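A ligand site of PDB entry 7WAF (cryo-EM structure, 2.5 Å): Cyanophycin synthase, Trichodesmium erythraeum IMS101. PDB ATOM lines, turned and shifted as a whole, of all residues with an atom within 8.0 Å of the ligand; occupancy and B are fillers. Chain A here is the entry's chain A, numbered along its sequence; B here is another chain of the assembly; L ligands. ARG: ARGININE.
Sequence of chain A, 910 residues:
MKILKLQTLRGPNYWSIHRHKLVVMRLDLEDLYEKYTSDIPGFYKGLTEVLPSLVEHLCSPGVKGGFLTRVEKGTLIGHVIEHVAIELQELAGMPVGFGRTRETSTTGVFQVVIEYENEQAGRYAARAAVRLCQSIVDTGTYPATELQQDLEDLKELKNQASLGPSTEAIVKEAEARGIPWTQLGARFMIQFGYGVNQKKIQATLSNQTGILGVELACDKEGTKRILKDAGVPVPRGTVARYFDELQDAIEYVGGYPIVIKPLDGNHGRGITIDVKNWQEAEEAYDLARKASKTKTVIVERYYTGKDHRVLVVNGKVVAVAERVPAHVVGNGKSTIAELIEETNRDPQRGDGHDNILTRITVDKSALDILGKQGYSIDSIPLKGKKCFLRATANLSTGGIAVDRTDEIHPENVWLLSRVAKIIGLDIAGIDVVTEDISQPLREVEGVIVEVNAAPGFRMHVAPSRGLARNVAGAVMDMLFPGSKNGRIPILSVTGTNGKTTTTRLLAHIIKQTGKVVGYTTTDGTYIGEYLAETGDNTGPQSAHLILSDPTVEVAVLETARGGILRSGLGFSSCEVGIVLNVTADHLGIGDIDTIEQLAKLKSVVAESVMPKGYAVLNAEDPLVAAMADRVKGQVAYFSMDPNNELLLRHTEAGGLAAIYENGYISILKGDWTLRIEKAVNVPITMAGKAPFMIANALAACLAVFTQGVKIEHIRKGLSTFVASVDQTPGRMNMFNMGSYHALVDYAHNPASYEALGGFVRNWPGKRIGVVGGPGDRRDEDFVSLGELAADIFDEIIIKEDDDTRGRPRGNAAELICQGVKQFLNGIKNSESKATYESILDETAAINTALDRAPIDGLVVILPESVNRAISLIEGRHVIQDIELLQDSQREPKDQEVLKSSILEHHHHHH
CA of Gly 164 touches OXT of the ligand, 3.6 Å away.
Phe 188 touches the ligand (CE2 to NH1, 3.9 Å).
Ala 203 touches the ligand.
His 353 touches the ligand.
Asp 2 of chain B touches the ligand.
Hydrophobic or aromatic side chains that line the ligand: Phe 188, Ala 203 and His 353.
Within 4 Å of the ligand: Gly 164, Ser 166, Thr 167, Phe 188, Ala 203, His 353, Asp 2 of chain B and Asp 3 of chain B.
Along chain A the residues within 4 Å of the ligand span positions 164 to 353.
The nearest printed residue that does not touch the ligand is Pro 165 (4.2 Å).
The side-chain hydroxyl (OG1) of Thr 167 sits at hydrogen-bond distance from an oxygen (OXT) of the ligand (3.5 Å).
A side-chain carbon (CG) of Asp 3 of chain B is bonded to a nitrogen (N) of the ligand (1.3 Å).
The side-chain hydroxyl of Ser 166 sits at hydrogen-bond distance from an oxygen (O) of the ligand (3.5 Å).
N of Asp 2 of chain B lies within hydrogen-bond range of OD1 of Asp 4 of chain B (3.2 Å).
OG1 of Thr 167 is in hydrogen-bond range of O of Gln 202 (3.4 Å).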
ATOM      1  N   GLN A 160      29.175  -8.361   9.390  1.00  0.00           N
ATOM      2  CA  GLN A 160      30.514  -8.166   8.845  1.00  0.00           C
ATOM      3  C   GLN A 160      30.610  -8.682   7.411  1.00  0.00           C
ATOM      4  O   GLN A 160      31.151  -8.004   6.535  1.00  0.00           O
ATOM      5  CB  GLN A 160      31.546  -8.854   9.732  1.00  0.00           C
ATOM      6  CG  GLN A 160      32.983  -8.590   9.340  1.00  0.00           C
ATOM      7  CD  GLN A 160      33.958  -9.391  10.186  1.00  0.00           C
ATOM      8  OE1 GLN A 160      33.585 -10.335  10.862  1.00  0.00           O
ATOM      9  NE2 GLN A 160      35.232  -8.996  10.144  1.00  0.00           N
ATOM     10  N   SER A 162      28.516  -8.890   4.947  1.00  0.00           N
ATOM     11  CA  SER A 162      27.322  -8.427   4.260  1.00  0.00           C
ATOM     12  C   SER A 162      27.696  -7.373   3.244  1.00  0.00           C
ATOM     13  O   SER A 162      28.531  -6.507   3.512  1.00  0.00           O
ATOM     14  CB  SER A 162      26.300  -7.860   5.248  1.00  0.00           C
ATOM     15  OG  SER A 162      25.276  -7.164   4.560  1.00  0.00           O
ATOM     16  N   LEU A 163      27.075  -7.437   2.072  1.00  0.00           N
ATOM     17  CA  LEU A 163      27.222  -6.389   1.081  1.00  0.00           C
ATOM     18  C   LEU A 163      26.385  -5.180   1.480  1.00  0.00           C
ATOM     19  O   LEU A 163      25.687  -5.191   2.491  1.00  0.00           O
ATOM     20  CB  LEU A 163      26.813  -6.899  -0.308  1.00  0.00           C
ATOM     21  CG  LEU A 163      27.219  -8.325  -0.663  1.00  0.00           C
ATOM     22  CD1 LEU A 163      26.544  -8.779  -1.950  1.00  0.00           C
ATOM     23  CD2 LEU A 163      28.720  -8.451  -0.769  1.00  0.00           C
ATOM     24  N   GLY A 164      26.485  -4.126   0.679  1.00  0.00           N
ATOM     25  CA  GLY A 164      25.645  -2.966   0.862  1.00  0.00           C
ATOM     26  C   GLY A 164      24.319  -3.124   0.147  1.00  0.00           C
ATOM     27  O   GLY A 164      24.160  -3.993  -0.705  1.00  0.00           O
ATOM     28  N   PRO A 165      23.343  -2.283   0.505  1.00  0.00           N
ATOM     29  CA  PRO A 165      22.035  -2.374  -0.173  1.00  0.00           C
ATOM     30  C   PRO A 165      22.102  -2.194  -1.684  1.00  0.00           C
ATOM     31  O   PRO A 165      21.343  -2.859  -2.396  1.00  0.00           O
ATOM     32  CB  PRO A 165      21.216  -1.253   0.491  1.00  0.00           C
ATOM     33  CG  PRO A 165      22.219  -0.407   1.214  1.00  0.00           C
ATOM     34  CD  PRO A 165      23.308  -1.336   1.620  1.00  0.00           C
ATOM     35  N   SER A 166      22.983  -1.332  -2.182  1.00  0.00           N
ATOM     36  CA  SER A 166      23.121  -1.192  -3.628  1.00  0.00           C
ATOM     37  C   SER A 166      23.671  -2.477  -4.252  1.00  0.00           C
ATOM     38  O   SER A 166      23.112  -3.012  -5.217  1.00  0.00           O
ATOM     39  CB  SER A 166      24.024  -0.010  -3.968  1.00  0.00           C
ATOM     40  OG  SER A 166      23.503   1.201  -3.436  1.00  0.00           O
ATOM     41  N   THR A 167      24.760  -2.988  -3.683  1.00  0.00           N
ATOM     42  CA  THR A 167      25.318  -4.248  -4.157  1.00  0.00           C
ATOM     43  C   THR A 167      24.339  -5.395  -3.935  1.00  0.00           C
ATOM     44  O   THR A 167      24.231  -6.281  -4.783  1.00  0.00           O
ATOM     45  CB  THR A 167      26.641  -4.543  -3.448  1.00  0.00           C
ATOM     46  OG1 THR A 167      27.442  -3.343  -3.409  1.00  0.00           O
ATOM     47  CG2 THR A 167      27.404  -5.620  -4.184  1.00  0.00           C
ATOM     48  N   GLU A 168      23.620  -5.385  -2.811  1.00  0.00           N
ATOM     49  CA  GLU A 168      22.616  -6.423  -2.572  1.00  0.00           C
ATOM     50  C   GLU A 168      21.544  -6.418  -3.658  1.00  0.00           C
ATOM     51  O   GLU A 168      21.183  -7.466  -4.185  1.00  0.00           O
ATOM     52  CB  GLU A 168      21.980  -6.254  -1.197  1.00  0.00           C
ATOM     53  CG  GLU A 168      22.764  -6.834  -0.041  1.00  0.00           C
ATOM     54  CD  GLU A 168      22.288  -6.303   1.295  1.00  0.00           C
ATOM     55  OE1 GLU A 168      23.133  -5.909   2.123  1.00  0.00           O
ATOM     56  OE2 GLU A 168      21.061  -6.271   1.519  1.00  0.00           O
ATOM     57  N   ILE A 170      21.705  -5.158  -6.739  1.00  0.00           N
ATOM     58  CA  ILE A 170      22.229  -5.524  -8.046  1.00  0.00           C
ATOM     59  C   ILE A 170      22.491  -7.028  -8.119  1.00  0.00           C
ATOM     60  O   ILE A 170      22.185  -7.682  -9.128  1.00  0.00           O
ATOM     61  CB  ILE A 170      23.492  -4.704  -8.368  1.00  0.00           C
ATOM     62  CG1 ILE A 170      23.131  -3.224  -8.501  1.00  0.00           C
ATOM     63  CG2 ILE A 170      24.155  -5.200  -9.637  1.00  0.00           C
ATOM     64  CD1 ILE A 170      24.310  -2.289  -8.423  1.00  0.00           C
ATOM     65  N   GLN A 183      32.406 -12.963  -5.641  1.00  0.00           N
ATOM     66  CA  GLN A 183      32.981 -11.865  -4.875  1.00  0.00           C
ATOM     67  C   GLN A 183      34.490 -11.889  -5.022  1.00  0.00           C
ATOM     68  O   GLN A 183      35.143 -12.854  -4.620  1.00  0.00           O
ATOM     69  CB  GLN A 183      32.577 -11.964  -3.401  1.00  0.00           C
ATOM     70  CG  GLN A 183      32.876 -10.712  -2.598  1.00  0.00           C
ATOM     71  CD  GLN A 183      31.956 -10.552  -1.414  1.00  0.00           C
ATOM     72  OE1 GLN A 183      31.193 -11.459  -1.081  1.00  0.00           O
ATOM     73  NE2 GLN A 183      32.030  -9.396  -0.767  1.00  0.00           N
ATOM     74  N   ARG A 187      38.691  -5.431  -3.483  1.00  0.00           N
ATOM     75  CA  ARG A 187      38.136  -4.120  -3.133  1.00  0.00           C
ATOM     76  C   ARG A 187      36.617  -4.186  -3.056  1.00  0.00           C
ATOM     77  O   ARG A 187      35.925  -3.267  -3.504  1.00  0.00           O
ATOM     78  CB  ARG A 187      38.570  -3.057  -4.127  1.00  0.00           C
ATOM     79  CG  ARG A 187      40.078  -2.896  -4.259  1.00  0.00           C
ATOM     80  CD  ARG A 187      40.427  -2.056  -5.464  1.00  0.00           C
ATOM     81  NE  ARG A 187      39.843  -0.733  -5.364  1.00  0.00           N
ATOM     82  CZ  ARG A 187      40.328   0.244  -4.614  1.00  0.00           C
ATOM     83  NH1 ARG A 187      41.423   0.081  -3.885  1.00  0.00           N
ATOM     84  NH2 ARG A 187      39.694   1.416  -4.582  1.00  0.00           N
ATOM     85  N   PHE A 188      36.078  -5.263  -2.494  1.00  0.00           N
ATOM     86  CA  PHE A 188      34.637  -5.485  -2.425  1.00  0.00           C
ATOM     87  C   PHE A 188      34.001  -5.427  -3.813  1.00  0.00           C
ATOM     88  O   PHE A 188      32.890  -4.929  -3.996  1.00  0.00           O
ATOM     89  CB  PHE A 188      33.972  -4.478  -1.481  1.00  0.00           C
ATOM     90  CG  PHE A 188      34.678  -4.313  -0.173  1.00  0.00           C
ATOM     91  CD1 PHE A 188      34.607  -5.287   0.804  1.00  0.00           C
ATOM     92  CD2 PHE A 188      35.431  -3.172   0.084  1.00  0.00           C
ATOM     93  CE1 PHE A 188      35.260  -5.138   2.008  1.00  0.00           C
ATOM     94  CE2 PHE A 188      36.084  -3.023   1.288  1.00  0.00           C
ATOM     95  CZ  PHE A 188      36.001  -3.995   2.252  1.00  0.00           C
ATOM     96  N   MET A 189      34.724  -5.945  -4.798  1.00  0.00           N
ATOM     97  CA  MET A 189      34.242  -5.968  -6.167  1.00  0.00           C
ATOM     98  C   MET A 189      33.506  -7.260  -6.460  1.00  0.00           C
ATOM     99  O   MET A 189      33.931  -8.340  -6.024  1.00  0.00           O
ATOM    100  CB  MET A 189      35.399  -5.785  -7.154  1.00  0.00           C
ATOM    101  CG  MET A 189      36.176  -4.505  -6.970  1.00  0.00           C
ATOM    102  SD  MET A 189      36.787  -3.835  -8.538  1.00  0.00           S
ATOM    103  CE  MET A 189      38.319  -4.732  -8.715  1.00  0.00           C
ATOM    104  N   GLN A 202      31.559  -2.299  -8.163  1.00  0.00           N
ATOM    105  CA  GLN A 202      31.944  -2.220  -6.757  1.00  0.00           C
ATOM    106  C   GLN A 202      30.727  -2.024  -5.861  1.00  0.00           C
ATOM    107  O   GLN A 202      30.374  -2.912  -5.078  1.00  0.00           O
ATOM    108  CB  GLN A 202      32.949  -1.090  -6.535  1.00  0.00           C
ATOM    109  CG  GLN A 202      33.703  -1.194  -5.230  1.00  0.00           C
ATOM    110  CD  GLN A 202      34.754  -0.117  -5.092  1.00  0.00           C
ATOM    111  OE1 GLN A 202      34.468   1.066  -5.250  1.00  0.00           O
ATOM    112  NE2 GLN A 202      35.984  -0.521  -4.800  1.00  0.00           N
ATOM    113  N   ALA A 203      30.076  -0.871  -5.979  1.00  0.00           N
ATOM    114  CA  ALA A 203      28.733  -0.652  -5.449  1.00  0.00           C
ATOM    115  C   ALA A 203      27.793  -0.179  -6.537  1.00  0.00           C
ATOM    116  O   ALA A 203      26.739  -0.794  -6.761  1.00  0.00           O
ATOM    117  CB  ALA A 203      28.771   0.334  -4.273  1.00  0.00           C
ATOM    118  N   THR A 204      28.151   0.901  -7.220  1.00  0.00           N
ATOM    119  CA  THR A 204      27.431   1.402  -8.382  1.00  0.00           C
ATOM    120  C   THR A 204      28.348   1.673  -9.555  1.00  0.00           C
ATOM    121  O   THR A 204      27.887   1.628 -10.709  1.00  0.00           O
ATOM    122  CB  THR A 204      26.654   2.681  -8.021  1.00  0.00           C
ATOM    123  OG1 THR A 204      25.866   2.439  -6.853  1.00  0.00           O
ATOM    124  CG2 THR A 204      25.726   3.075  -9.144  1.00  0.00           C
ATOM    125  N   HIS A 353      22.014   1.476   8.038  1.00  0.00           N
ATOM    126  CA  HIS A 353      22.175   1.752   6.612  1.00  0.00           C
ATOM    127  C   HIS A 353      21.251   0.875   5.781  1.00  0.00           C
ATOM    128  O   HIS A 353      21.471   0.692   4.575  1.00  0.00           O
ATOM    129  CB  HIS A 353      23.645   1.573   6.212  1.00  0.00           C
ATOM    130  CG  HIS A 353      23.969   1.996   4.820  1.00  0.00           C
ATOM    131  ND1 HIS A 353      23.841   1.165   3.732  1.00  0.00           N
ATOM    132  CD2 HIS A 353      24.415   3.180   4.335  1.00  0.00           C
ATOM    133  CE1 HIS A 353      24.199   1.814   2.636  1.00  0.00           C
ATOM    134  NE2 HIS A 353      24.551   3.037   2.979  1.00  0.00           N
ATOM    135  N   ALA A 454      28.857   7.180  -8.743  1.00  0.00           N
ATOM    136  CA  ALA A 454      28.477   6.118  -7.812  1.00  0.00           C
ATOM    137  C   ALA A 454      27.345   6.555  -6.887  1.00  0.00           C
ATOM    138  O   ALA A 454      27.488   6.534  -5.663  1.00  0.00           O
ATOM    139  CB  ALA A 454      29.679   5.649  -7.001  1.00  0.00           C
ATOM    140  N   PRO A 455      26.201   6.969  -7.432  1.00  0.00           N
ATOM    141  CA  PRO A 455      25.103   7.416  -6.582  1.00  0.00           C
ATOM    142  C   PRO A 455      24.400   6.252  -5.907  1.00  0.00           C
ATOM    143  O   PRO A 455      24.416   5.125  -6.380  1.00  0.00           O
ATOM    144  CB  PRO A 455      24.173   8.132  -7.570  1.00  0.00           C
ATOM    145  CG  PRO A 455      24.376   7.402  -8.833  1.00  0.00           C
ATOM    146  CD  PRO A 455      25.802   6.905  -8.847  1.00  0.00           C
ATOM    147  N   GLY A 456      23.773   6.558  -4.773  1.00  0.00           N
ATOM    148  CA  GLY A 456      22.927   5.597  -4.102  1.00  0.00           C
ATOM    149  C   GLY A 456      21.491   5.725  -4.584  1.00  0.00           C
ATOM    150  O   GLY A 456      20.903   6.797  -4.532  1.00  0.00           O
ATOM    151  N   PHE A 457      20.953   4.608  -5.059  1.00  0.00           N
ATOM    152  CA  PHE A 457      19.572   4.553  -5.536  1.00  0.00           C
ATOM    153  C   PHE A 457      18.636   4.042  -4.443  1.00  0.00           C
ATOM    154  O   PHE A 457      17.556   3.537  -4.732  1.00  0.00           O
ATOM    155  CB  PHE A 457      19.466   3.687  -6.781  1.00  0.00           C
ATOM    156  CG  PHE A 457      20.082   2.322  -6.627  1.00  0.00           C
ATOM    157  CD1 PHE A 457      19.381   1.286  -6.062  1.00  0.00           C
ATOM    158  CD2 PHE A 457      21.376   2.091  -7.075  1.00  0.00           C
ATOM    159  CE1 PHE A 457      19.943   0.027  -5.927  1.00  0.00           C
ATOM    160  CE2 PHE A 457      21.945   0.842  -6.947  1.00  0.00           C
ATOM    161  CZ  PHE A 457      21.228  -0.184  -6.372  1.00  0.00           C
ATOM    162  N   ARG A 458      19.058   4.195  -3.192  1.00  0.00           N
ATOM    163  CA  ARG A 458      18.302   3.634  -2.080  1.00  0.00           C
ATOM    164  C   ARG A 458      16.969   4.348  -1.896  1.00  0.00           C
ATOM    165  O   ARG A 458      16.024   3.767  -1.354  1.00  0.00           O
ATOM    166  CB  ARG A 458      19.158   3.713  -0.816  1.00  0.00           C
ATOM    167  CG  ARG A 458      18.648   2.901   0.348  1.00  0.00           C
ATOM    168  CD  ARG A 458      19.694   2.819   1.446  1.00  0.00           C
ATOM    169  NE  ARG A 458      20.565   3.992   1.470  1.00  0.00           N
ATOM    170  CZ  ARG A 458      20.437   5.017   2.296  1.00  0.00           C
ATOM    171  NH1 ARG A 458      19.472   5.047   3.211  1.00  0.00           N
ATOM    172  NH2 ARG A 458      21.279   6.032   2.213  1.00  0.00           N
ATOM    173  N   ASP B   1      31.684  10.323   0.596  1.00  0.00           N
ATOM    174  CA  ASP B   1      32.248   9.429  -0.435  1.00  0.00           C
ATOM    175  C   ASP B   1      31.598   8.052  -0.319  1.00  0.00           C
ATOM    176  O   ASP B   1      31.247   7.600   0.776  1.00  0.00           O
ATOM    177  CB  ASP B   1      33.756   9.295  -0.284  1.00  0.00           C
ATOM    178  N   ASP B   2      31.454   7.389  -1.469  1.00  0.00           N
ATOM    179  CA  ASP B   2      30.861   6.049  -1.532  1.00  0.00           C
ATOM    180  C   ASP B   2      29.348   6.160  -1.307  1.00  0.00           C
ATOM    181  O   ASP B   2      28.890   6.591  -0.246  1.00  0.00           O
ATOM    182  CB  ASP B   2      31.464   5.162  -0.453  1.00  0.00           C
ATOM    183  N   ASP B   3      28.589   5.777  -2.346  1.00  0.00           N
ATOM    184  CA  ASP B   3      27.119   5.832  -2.311  1.00  0.00           C
ATOM    185  C   ASP B   3      26.666   7.280  -2.145  1.00  0.00           C
ATOM    186  O   ASP B   3      25.909   7.604  -1.224  1.00  0.00           O
ATOM    187  CB  ASP B   3      26.612   4.976  -1.144  1.00  0.00           C
ATOM    188  CG  ASP B   3      26.923   3.499  -1.431  1.00  0.00           C
ATOM    189  OD1 ASP B   3      26.512   2.954  -2.457  1.00  0.00           O
ATOM    190  N   ASP B   4      27.138   8.124  -3.062  1.00  0.00           N
ATOM    191  CA  ASP B   4      26.813   9.555  -3.054  1.00  0.00           C
ATOM    192  C   ASP B   4      25.399   9.756  -3.611  1.00  0.00           C
ATOM    193  O   ASP B   4      24.476   9.139  -3.051  1.00  0.00           O
ATOM    194  CB  ASP B   4      27.823  10.308  -3.924  1.00  0.00           C
ATOM    195  CG  ASP B   4      29.244   9.975  -3.475  1.00  0.00           C
ATOM    196  OD1 ASP B   4      29.501   9.762  -2.290  1.00  0.00           O
ATOM    197  OXT ASP B   4      25.276  10.531  -4.594  1.00  0.00           O
HETATM  198  N   ARG L   1      27.668   2.889  -0.493  1.00  0.00           N
HETATM  199  CA  ARG L   1      28.062   1.479  -0.620  1.00  0.00           C
HETATM  200  C   ARG L   1      26.838   0.617  -0.928  1.00  0.00           C
HETATM  201  O   ARG L   1      25.716   1.131  -0.760  1.00  0.00           O
HETATM  202  CB  ARG L   1      28.689   1.006   0.697  1.00  0.00           C
HETATM  203  CG  ARG L   1      28.872  -0.515   0.670  1.00  0.00           C
HETATM  204  CD  ARG L   1      30.223  -0.848   0.058  1.00  0.00           C
HETATM  205  NE  ARG L   1      31.291  -0.656   1.047  1.00  0.00           N
HETATM  206  CZ  ARG L   1      31.860  -1.644   1.740  1.00  0.00           C
HETATM  207  NH1 ARG L   1      32.823  -1.374   2.636  1.00  0.00           N
HETATM  208  NH2 ARG L   1      31.465  -2.920   1.545  1.00  0.00           N
HETATM  209  OXT ARG L   1      27.056  -0.551  -1.345  1.00  0.00           O
